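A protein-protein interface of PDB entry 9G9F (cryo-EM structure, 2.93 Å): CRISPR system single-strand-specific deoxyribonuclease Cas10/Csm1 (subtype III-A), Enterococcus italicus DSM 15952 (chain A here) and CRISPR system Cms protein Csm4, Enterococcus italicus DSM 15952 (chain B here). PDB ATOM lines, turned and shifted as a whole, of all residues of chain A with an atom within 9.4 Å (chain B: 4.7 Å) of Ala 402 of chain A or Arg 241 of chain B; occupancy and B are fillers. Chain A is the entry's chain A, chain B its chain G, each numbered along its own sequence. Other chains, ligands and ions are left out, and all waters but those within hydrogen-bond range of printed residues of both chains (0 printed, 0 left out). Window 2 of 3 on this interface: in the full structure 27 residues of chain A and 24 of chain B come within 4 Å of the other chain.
O of Tyr 405 of chain A is in hydrogen-bond range of OH of Tyr 242 of chain B (3.0 Å).
The backbone carbonyl oxygen of Tyr 242 of chain B lies close to the backbone carbonyl oxygen of Ala 402 of chain A, 3.2 Å away.
O of His 403 of chain A is in hydrogen-bond range of OH of Tyr 242 of chain B (3.0 Å).
NH1 of Arg 241 of chain B lies within salt-bridge range of OD1 of Asp 399 of chain A, 3.4 Å away.
ND1 of His 403 of chain A sits at hydrogen-bond distance from O of Ala 240 of chain B.
The backbone carbonyl oxygen (O) of Arg 241 of chain B sits at hydrogen-bond distance from the backbone NH (N) of Thr 274 of chain B, 2.8 Å away.
O of Tyr 405 of chain A lies close to NE2 of His 403 of chain A (3.0 Å).
The guanidinium group (NE) of Arg 395 of chain A lies within salt-bridge range of the side-chain carboxylate (OD2) of Asp 399 of chain A (3.98 Å).
OG of Ser 398 of chain A touches NH2 of Arg 241 of chain B, at 3.9 Å.
Asp 399 of chain A touches Arg 79 of chain B (OD1 to CG, 3.7 Å).
Ala 402 of chain A touches Arg 241 of chain B (CB to NH2, 3.4 Å).
Of chain B, only Arg 241 and Tyr 242 come within 4 Å of Ala 402 of chain A.
Ala 240 of chain B touches just one residue of chain A: His 403.
No residue of chain A comes within 4 Å of Ser 273 of chain B.
Printed residues of chain B within 4 Å of Ser 398 of chain A: Arg 241.
Of the printed residues of chain B, Tyr 405 of chain A touches Tyr 242 (3.0 Å).
Of the printed residues of chain B, Asp 399 of chain A touches Arg 79 and Arg 241.
The nearest printed residue of chain B that does not touch Ala 402 of chain A is Ala 240 of chain B (5.0 Å).
Hydrophobic or aromatic side chains of chain B that line the printed part of chain A: Tyr 242.
Of the 18 printed residues of chain A, 5 touch a printed residue of chain B.
Hydrophobic or aromatic side chains of chain A that line the printed part of chain B: Ala 402, His 403 and Tyr 405.
Among the printed residues, 8 pairs touch across the chains.
Among the printed residues, Asp or Glu carboxylates within 4 Å of a Lys or Arg side-chain nitrogen of the other chain: Asp 399 of chain A with Arg 241 of chain B (3.4 Å).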
ATOM      1  N   ASP A 275      14.650  -4.456  -1.874  1.00  0.00           N
ATOM      2  CA  ASP A 275      15.535  -3.347  -1.555  1.00  0.00           C
ATOM      3  C   ASP A 275      16.610  -3.234  -2.624  1.00  0.00           C
ATOM      4  O   ASP A 275      17.045  -4.240  -3.190  1.00  0.00           O
ATOM      5  CB  ASP A 275      16.176  -3.534  -0.173  1.00  0.00           C
ATOM      6  CG  ASP A 275      17.225  -2.477   0.141  1.00  0.00           C
ATOM      7  OD1 ASP A 275      16.965  -1.280  -0.093  1.00  0.00           O
ATOM      8  OD2 ASP A 275      18.308  -2.844   0.639  1.00  0.00           O
ATOM      9  N   SER A 277      20.413  -2.269  -3.739  1.00  0.00           N
ATOM     10  CA  SER A 277      21.747  -2.302  -3.162  1.00  0.00           C
ATOM     11  C   SER A 277      22.677  -1.429  -3.990  1.00  0.00           C
ATOM     12  O   SER A 277      22.672  -1.504  -5.222  1.00  0.00           O
ATOM     13  CB  SER A 277      22.275  -3.735  -3.104  1.00  0.00           C
ATOM     14  OG  SER A 277      21.281  -4.618  -2.615  1.00  0.00           O
ATOM     15  N   LYS A 354      17.522 -10.004 -11.513  1.00  0.00           N
ATOM     16  CA  LYS A 354      18.918 -10.192 -11.142  1.00  0.00           C
ATOM     17  C   LYS A 354      19.801 -10.274 -12.381  1.00  0.00           C
ATOM     18  O   LYS A 354      20.859  -9.637 -12.449  1.00  0.00           O
ATOM     19  CB  LYS A 354      19.053 -11.451 -10.285  1.00  0.00           C
ATOM     20  CG  LYS A 354      20.474 -11.830  -9.927  1.00  0.00           C
ATOM     21  CD  LYS A 354      20.514 -13.129  -9.132  1.00  0.00           C
ATOM     22  CE  LYS A 354      19.716 -13.039  -7.841  1.00  0.00           C
ATOM     23  NZ  LYS A 354      19.831 -11.706  -7.187  1.00  0.00           N
ATOM     24  N   ALA A 368      17.351  -7.189  -4.094  1.00  0.00           N
ATOM     25  CA  ALA A 368      17.104  -8.419  -3.358  1.00  0.00           C
ATOM     26  C   ALA A 368      15.658  -8.414  -2.893  1.00  0.00           C
ATOM     27  O   ALA A 368      15.184  -7.416  -2.344  1.00  0.00           O
ATOM     28  CB  ALA A 368      18.054  -8.560  -2.169  1.00  0.00           C
ATOM     29  N   SER A 394      12.566  -8.595   7.087  1.00  0.00           N
ATOM     30  CA  SER A 394      13.817  -7.851   6.985  1.00  0.00           C
ATOM     31  C   SER A 394      15.026  -8.769   7.129  1.00  0.00           C
ATOM     32  O   SER A 394      16.031  -8.591   6.435  1.00  0.00           O
ATOM     33  CB  SER A 394      13.860  -6.741   8.032  1.00  0.00           C
ATOM     34  OG  SER A 394      14.771  -5.728   7.651  1.00  0.00           O
ATOM     35  N   ARG A 395      14.954  -9.751   8.029  1.00  0.00           N
ATOM     36  CA  ARG A 395      16.062 -10.689   8.189  1.00  0.00           C
ATOM     37  C   ARG A 395      16.263 -11.534   6.936  1.00  0.00           C
ATOM     38  O   ARG A 395      17.404 -11.782   6.522  1.00  0.00           O
ATOM     39  CB  ARG A 395      15.815 -11.581   9.404  1.00  0.00           C
ATOM     40  CG  ARG A 395      17.006 -12.429   9.806  1.00  0.00           C
ATOM     41  CD  ARG A 395      16.561 -13.815  10.236  1.00  0.00           C
ATOM     42  NE  ARG A 395      16.047 -14.591   9.113  1.00  0.00           N
ATOM     43  CZ  ARG A 395      15.347 -15.709   9.235  1.00  0.00           C
ATOM     44  NH1 ARG A 395      15.044 -16.210  10.421  1.00  0.00           N
ATOM     45  NH2 ARG A 395      14.935 -16.339   8.139  1.00  0.00           N
ATOM     46  N   LYS A 396      15.169 -11.993   6.322  1.00  0.00           N
ATOM     47  CA  LYS A 396      15.289 -12.738   5.072  1.00  0.00           C
ATOM     48  C   LYS A 396      15.893 -11.871   3.975  1.00  0.00           C
ATOM     49  O   LYS A 396      16.736 -12.334   3.195  1.00  0.00           O
ATOM     50  CB  LYS A 396      13.924 -13.267   4.639  1.00  0.00           C
ATOM     51  CG  LYS A 396      13.368 -14.368   5.515  1.00  0.00           C
ATOM     52  CD  LYS A 396      12.041 -14.866   4.972  1.00  0.00           C
ATOM     53  CE  LYS A 396      11.507 -16.022   5.793  1.00  0.00           C
ATOM     54  NZ  LYS A 396      12.411 -17.200   5.748  1.00  0.00           N
ATOM     55  N   LEU A 397      15.469 -10.608   3.900  1.00  0.00           N
ATOM     56  CA  LEU A 397      16.045  -9.692   2.923  1.00  0.00           C
ATOM     57  C   LEU A 397      17.536  -9.508   3.160  1.00  0.00           C
ATOM     58  O   LEU A 397      18.323  -9.474   2.210  1.00  0.00           O
ATOM     59  CB  LEU A 397      15.323  -8.347   2.979  1.00  0.00           C
ATOM     60  CG  LEU A 397      15.945  -7.186   2.207  1.00  0.00           C
ATOM     61  CD1 LEU A 397      16.034  -7.516   0.737  1.00  0.00           C
ATOM     62  CD2 LEU A 397      15.147  -5.916   2.418  1.00  0.00           C
ATOM     63  N   SER A 398      17.943  -9.390   4.425  1.00  0.00           N
ATOM     64  CA  SER A 398      19.360  -9.241   4.741  1.00  0.00           C
ATOM     65  C   SER A 398      20.159 -10.468   4.327  1.00  0.00           C
ATOM     66  O   SER A 398      21.257 -10.343   3.779  1.00  0.00           O
ATOM     67  CB  SER A 398      19.542  -8.970   6.233  1.00  0.00           C
ATOM     68  OG  SER A 398      20.745  -9.551   6.700  1.00  0.00           O
ATOM     69  N   ASP A 399      19.631 -11.665   4.587  1.00  0.00           N
ATOM     70  CA  ASP A 399      20.338 -12.881   4.183  1.00  0.00           C
ATOM     71  C   ASP A 399      20.486 -12.952   2.667  1.00  0.00           C
ATOM     72  O   ASP A 399      21.566 -13.264   2.142  1.00  0.00           O
ATOM     73  CB  ASP A 399      19.605 -14.117   4.706  1.00  0.00           C
ATOM     74  CG  ASP A 399      19.629 -14.215   6.216  1.00  0.00           C
ATOM     75  OD1 ASP A 399      20.100 -13.263   6.871  1.00  0.00           O
ATOM     76  OD2 ASP A 399      19.177 -15.249   6.749  1.00  0.00           O
ATOM     77  N   LYS A 400      19.403 -12.655   1.944  1.00  0.00           N
ATOM     78  CA  LYS A 400      19.458 -12.692   0.487  1.00  0.00           C
ATOM     79  C   LYS A 400      20.398 -11.630  -0.063  1.00  0.00           C
ATOM     80  O   LYS A 400      21.043 -11.848  -1.093  1.00  0.00           O
ATOM     81  CB  LYS A 400      18.056 -12.525  -0.096  1.00  0.00           C
ATOM     82  CG  LYS A 400      17.922 -13.014  -1.523  1.00  0.00           C
ATOM     83  CD  LYS A 400      16.470 -13.240  -1.889  1.00  0.00           C
ATOM     84  CE  LYS A 400      15.823 -14.233  -0.944  1.00  0.00           C
ATOM     85  NZ  LYS A 400      14.378 -14.422  -1.239  1.00  0.00           N
ATOM     86  N   LYS A 401      20.487 -10.480   0.605  1.00  0.00           N
ATOM     87  CA  LYS A 401      21.437  -9.454   0.201  1.00  0.00           C
ATOM     88  C   LYS A 401      22.866  -9.862   0.523  1.00  0.00           C
ATOM     89  O   LYS A 401      23.804  -9.423  -0.151  1.00  0.00           O
ATOM     90  CB  LYS A 401      21.090  -8.138   0.889  1.00  0.00           C
ATOM     91  CG  LYS A 401      21.776  -6.926   0.313  1.00  0.00           C
ATOM     92  CD  LYS A 401      21.458  -5.693   1.136  1.00  0.00           C
ATOM     93  CE  LYS A 401      19.965  -5.545   1.347  1.00  0.00           C
ATOM     94  NZ  LYS A 401      19.238  -5.503   0.053  1.00  0.00           N
ATOM     95  N   ALA A 402      23.053 -10.684   1.555  1.00  0.00           N
ATOM     96  CA  ALA A 402      24.390 -11.165   1.883  1.00  0.00           C
ATOM     97  C   ALA A 402      24.894 -12.147   0.836  1.00  0.00           C
ATOM     98  O   ALA A 402      26.031 -12.034   0.369  1.00  0.00           O
ATOM     99  CB  ALA A 402      24.398 -11.803   3.270  1.00  0.00           C
ATOM    100  N   HIS A 403      24.067 -13.120   0.445  1.00  0.00           N
ATOM    101  CA  HIS A 403      24.520 -14.070  -0.573  1.00  0.00           C
ATOM    102  C   HIS A 403      24.609 -13.402  -1.943  1.00  0.00           C
ATOM    103  O   HIS A 403      25.693 -13.301  -2.525  1.00  0.00           O
ATOM    104  CB  HIS A 403      23.596 -15.285  -0.626  1.00  0.00           C
ATOM    105  CG  HIS A 403      24.152 -16.426  -1.419  1.00  0.00           C
ATOM    106  ND1 HIS A 403      25.268 -17.133  -1.027  1.00  0.00           N
ATOM    107  CD2 HIS A 403      23.746 -16.983  -2.584  1.00  0.00           C
ATOM    108  CE1 HIS A 403      25.524 -18.076  -1.916  1.00  0.00           C
ATOM    109  NE2 HIS A 403      24.616 -18.007  -2.870  1.00  0.00           N
ATOM    110  N   LYS A 404      23.471 -12.971  -2.485  1.00  0.00           N
ATOM    111  CA  LYS A 404      23.399 -11.974  -3.551  1.00  0.00           C
ATOM    112  C   LYS A 404      23.839 -12.446  -4.935  1.00  0.00           C
ATOM    113  O   LYS A 404      23.647 -11.716  -5.912  1.00  0.00           O
ATOM    114  CB  LYS A 404      24.223 -10.744  -3.161  1.00  0.00           C
ATOM    115  CG  LYS A 404      23.747  -9.447  -3.774  1.00  0.00           C
ATOM    116  CD  LYS A 404      24.513  -8.278  -3.197  1.00  0.00           C
ATOM    117  CE  LYS A 404      24.072  -6.969  -3.814  1.00  0.00           C
ATOM    118  NZ  LYS A 404      24.823  -5.826  -3.234  1.00  0.00           N
ATOM    119  N   TYR A 405      24.394 -13.650  -5.060  1.00  0.00           N
ATOM    120  CA  TYR A 405      24.877 -14.115  -6.356  1.00  0.00           C
ATOM    121  C   TYR A 405      24.864 -15.634  -6.385  1.00  0.00           C
ATOM    122  O   TYR A 405      24.721 -16.296  -5.357  1.00  0.00           O
ATOM    123  CB  TYR A 405      26.285 -13.588  -6.666  1.00  0.00           C
ATOM    124  CG  TYR A 405      26.312 -12.140  -7.094  1.00  0.00           C
ATOM    125  CD1 TYR A 405      25.640 -11.719  -8.228  1.00  0.00           C
ATOM    126  CD2 TYR A 405      27.001 -11.193  -6.354  1.00  0.00           C
ATOM    127  CE1 TYR A 405      25.654 -10.397  -8.611  1.00  0.00           C
ATOM    128  CE2 TYR A 405      27.023  -9.871  -6.733  1.00  0.00           C
ATOM    129  CZ  TYR A 405      26.348  -9.479  -7.862  1.00  0.00           C
ATOM    130  OH  TYR A 405      26.365  -8.162  -8.247  1.00  0.00           O
ATOM    131  N   SER A 406      25.016 -16.185  -7.587  1.00  0.00           N
ATOM    132  CA  SER A 406      25.002 -17.623  -7.801  1.00  0.00           C
ATOM    133  C   SER A 406      26.269 -18.031  -8.544  1.00  0.00           C
ATOM    134  O   SER A 406      27.053 -17.189  -8.985  1.00  0.00           O
ATOM    135  CB  SER A 406      23.748 -18.054  -8.571  1.00  0.00           C
ATOM    136  OG  SER A 406      23.656 -19.465  -8.654  1.00  0.00           O
ATOM    137  N   ILE A 410      28.785 -15.751 -11.109  1.00  0.00           N
ATOM    138  CA  ILE A 410      30.190 -15.534 -10.772  1.00  0.00           C
ATOM    139  C   ILE A 410      31.093 -16.005 -11.905  1.00  0.00           C
ATOM    140  O   ILE A 410      32.055 -15.320 -12.281  1.00  0.00           O
ATOM    141  CB  ILE A 410      30.540 -16.233  -9.448  1.00  0.00           C
ATOM    142  CG1 ILE A 410      29.760 -15.618  -8.290  1.00  0.00           C
ATOM    143  CG2 ILE A 410      32.024 -16.138  -9.181  1.00  0.00           C
ATOM    144  CD1 ILE A 410      30.040 -16.277  -6.961  1.00  0.00           C
ATOM    145  N   LEU B  77      31.258 -11.803   7.993  1.00  0.00           N
ATOM    146  CA  LEU B  77      29.886 -11.607   7.535  1.00  0.00           C
ATOM    147  C   LEU B  77      29.067 -12.789   8.028  1.00  0.00           C
ATOM    148  O   LEU B  77      29.002 -13.840   7.392  1.00  0.00           O
ATOM    149  CB  LEU B  77      29.832 -11.462   6.021  1.00  0.00           C
ATOM    150  CG  LEU B  77      30.532 -10.232   5.441  1.00  0.00           C
ATOM    151  CD1 LEU B  77      30.102 -10.006   4.011  1.00  0.00           C
ATOM    152  CD2 LEU B  77      30.252  -9.003   6.279  1.00  0.00           C
ATOM    153  N   ILE B  78      28.439 -12.614   9.191  1.00  0.00           N
ATOM    154  CA  ILE B  78      27.600 -13.635   9.801  1.00  0.00           C
ATOM    155  C   ILE B  78      26.257 -13.011  10.151  1.00  0.00           C
ATOM    156  O   ILE B  78      26.124 -11.792  10.275  1.00  0.00           O
ATOM    157  CB  ILE B  78      28.245 -14.252  11.058  1.00  0.00           C
ATOM    158  CG1 ILE B  78      28.686 -13.150  12.018  1.00  0.00           C
ATOM    159  CG2 ILE B  78      29.414 -15.137  10.680  1.00  0.00           C
ATOM    160  CD1 ILE B  78      29.254 -13.667  13.310  1.00  0.00           C
ATOM    161  N   ARG B  79      25.255 -13.870  10.305  1.00  0.00           N
ATOM    162  CA  ARG B  79      23.915 -13.404  10.622  1.00  0.00           C
ATOM    163  C   ARG B  79      23.861 -12.837  12.035  1.00  0.00           C
ATOM    164  O   ARG B  79      24.544 -13.309  12.947  1.00  0.00           O
ATOM    165  CB  ARG B  79      22.904 -14.541  10.474  1.00  0.00           C
ATOM    166  CG  ARG B  79      21.495 -14.076  10.153  1.00  0.00           C
ATOM    167  CD  ARG B  79      20.499 -15.212  10.282  1.00  0.00           C
ATOM    168  NE  ARG B  79      20.463 -15.746  11.638  1.00  0.00           N
ATOM    169  CZ  ARG B  79      19.686 -16.747  12.028  1.00  0.00           C
ATOM    170  NH1 ARG B  79      18.862 -17.351  11.188  1.00  0.00           N
ATOM    171  NH2 ARG B  79      19.735 -17.150  13.295  1.00  0.00           N
ATOM    172  N   ASP B 239      25.268 -21.934   1.170  1.00  0.00           N
ATOM    173  CA  ASP B 239      24.747 -21.038   2.218  1.00  0.00           C
ATOM    174  C   ASP B 239      25.860 -20.254   2.913  1.00  0.00           C
ATOM    175  O   ASP B 239      26.022 -20.286   4.133  1.00  0.00           O
ATOM    176  CB  ASP B 239      23.849 -21.786   3.220  1.00  0.00           C
ATOM    177  CG  ASP B 239      24.557 -22.899   3.992  1.00  0.00           C
ATOM    178  OD1 ASP B 239      25.792 -23.030   3.943  1.00  0.00           O
ATOM    179  OD2 ASP B 239      23.843 -23.669   4.666  1.00  0.00           O
ATOM    180  N   ALA B 240      26.626 -19.529   2.106  1.00  0.00           N
ATOM    181  CA  ALA B 240      27.758 -18.747   2.576  1.00  0.00           C
ATOM    182  C   ALA B 240      27.509 -17.273   2.301  1.00  0.00           C
ATOM    183  O   ALA B 240      26.911 -16.917   1.284  1.00  0.00           O
ATOM    184  CB  ALA B 240      29.051 -19.193   1.895  1.00  0.00           C
ATOM    185  N   ARG B 241      27.966 -16.421   3.209  1.00  0.00           N
ATOM    186  CA  ARG B 241      27.782 -14.983   3.097  1.00  0.00           C
ATOM    187  C   ARG B 241      29.100 -14.346   2.690  1.00  0.00           C
ATOM    188  O   ARG B 241      30.140 -14.638   3.285  1.00  0.00           O
ATOM    189  CB  ARG B 241      27.287 -14.401   4.418  1.00  0.00           C
ATOM    190  CG  ARG B 241      26.258 -15.274   5.112  1.00  0.00           C
ATOM    191  CD  ARG B 241      26.031 -14.837   6.541  1.00  0.00           C
ATOM    192  NE  ARG B 241      25.494 -13.487   6.611  1.00  0.00           N
ATOM    193  CZ  ARG B 241      24.206 -13.193   6.511  1.00  0.00           C
ATOM    194  NH1 ARG B 241      23.298 -14.135   6.324  1.00  0.00           N
ATOM    195  NH2 ARG B 241      23.821 -11.924   6.597  1.00  0.00           N
ATOM    196  N   TYR B 242      29.059 -13.485   1.678  1.00  0.00           N
ATOM    197  CA  TYR B 242      30.280 -12.925   1.120  1.00  0.00           C
ATOM    198  C   TYR B 242      29.994 -11.535   0.570  1.00  0.00           C
ATOM    199  O   TYR B 242      28.956 -10.933   0.854  1.00  0.00           O
ATOM    200  CB  TYR B 242      30.853 -13.855   0.047  1.00  0.00           C
ATOM    201  CG  TYR B 242      29.881 -14.230  -1.045  1.00  0.00           C
ATOM    202  CD1 TYR B 242      29.567 -13.340  -2.060  1.00  0.00           C
ATOM    203  CD2 TYR B 242      29.303 -15.487  -1.077  1.00  0.00           C
ATOM    204  CE1 TYR B 242      28.692 -13.683  -3.060  1.00  0.00           C
ATOM    205  CE2 TYR B 242      28.429 -15.839  -2.077  1.00  0.00           C
ATOM    206  CZ  TYR B 242      28.128 -14.934  -3.063  1.00  0.00           C
ATOM    207  OH  TYR B 242      27.252 -15.285  -4.060  1.00  0.00           O
ATOM    208  N   SER B 273      34.535 -12.550   4.306  1.00  0.00           N
ATOM    209  CA  SER B 273      33.472 -13.430   3.847  1.00  0.00           C
ATOM    210  C   SER B 273      33.560 -14.780   4.539  1.00  0.00           C
ATOM    211  O   SER B 273      34.647 -15.312   4.768  1.00  0.00           O
ATOM    212  CB  SER B 273      33.559 -13.606   2.337  1.00  0.00           C
ATOM    213  OG  SER B 273      33.532 -12.351   1.688  1.00  0.00           O
ATOM    214  N   THR B 274      32.402 -15.338   4.870  1.00  0.00           N
ATOM    215  CA  THR B 274      32.313 -16.590   5.607  1.00  0.00           C
ATOM    216  C   THR B 274      31.858 -17.712   4.688  1.00  0.00           C
ATOM    217  O   THR B 274      30.832 -17.589   4.012  1.00  0.00           O
ATOM    218  CB  THR B 274      31.343 -16.456   6.775  1.00  0.00           C
ATOM    219  OG1 THR B 274      31.502 -15.170   7.384  1.00  0.00           O
ATOM    220  CG2 THR B 274      31.611 -17.527   7.787  1.00  0.00           C
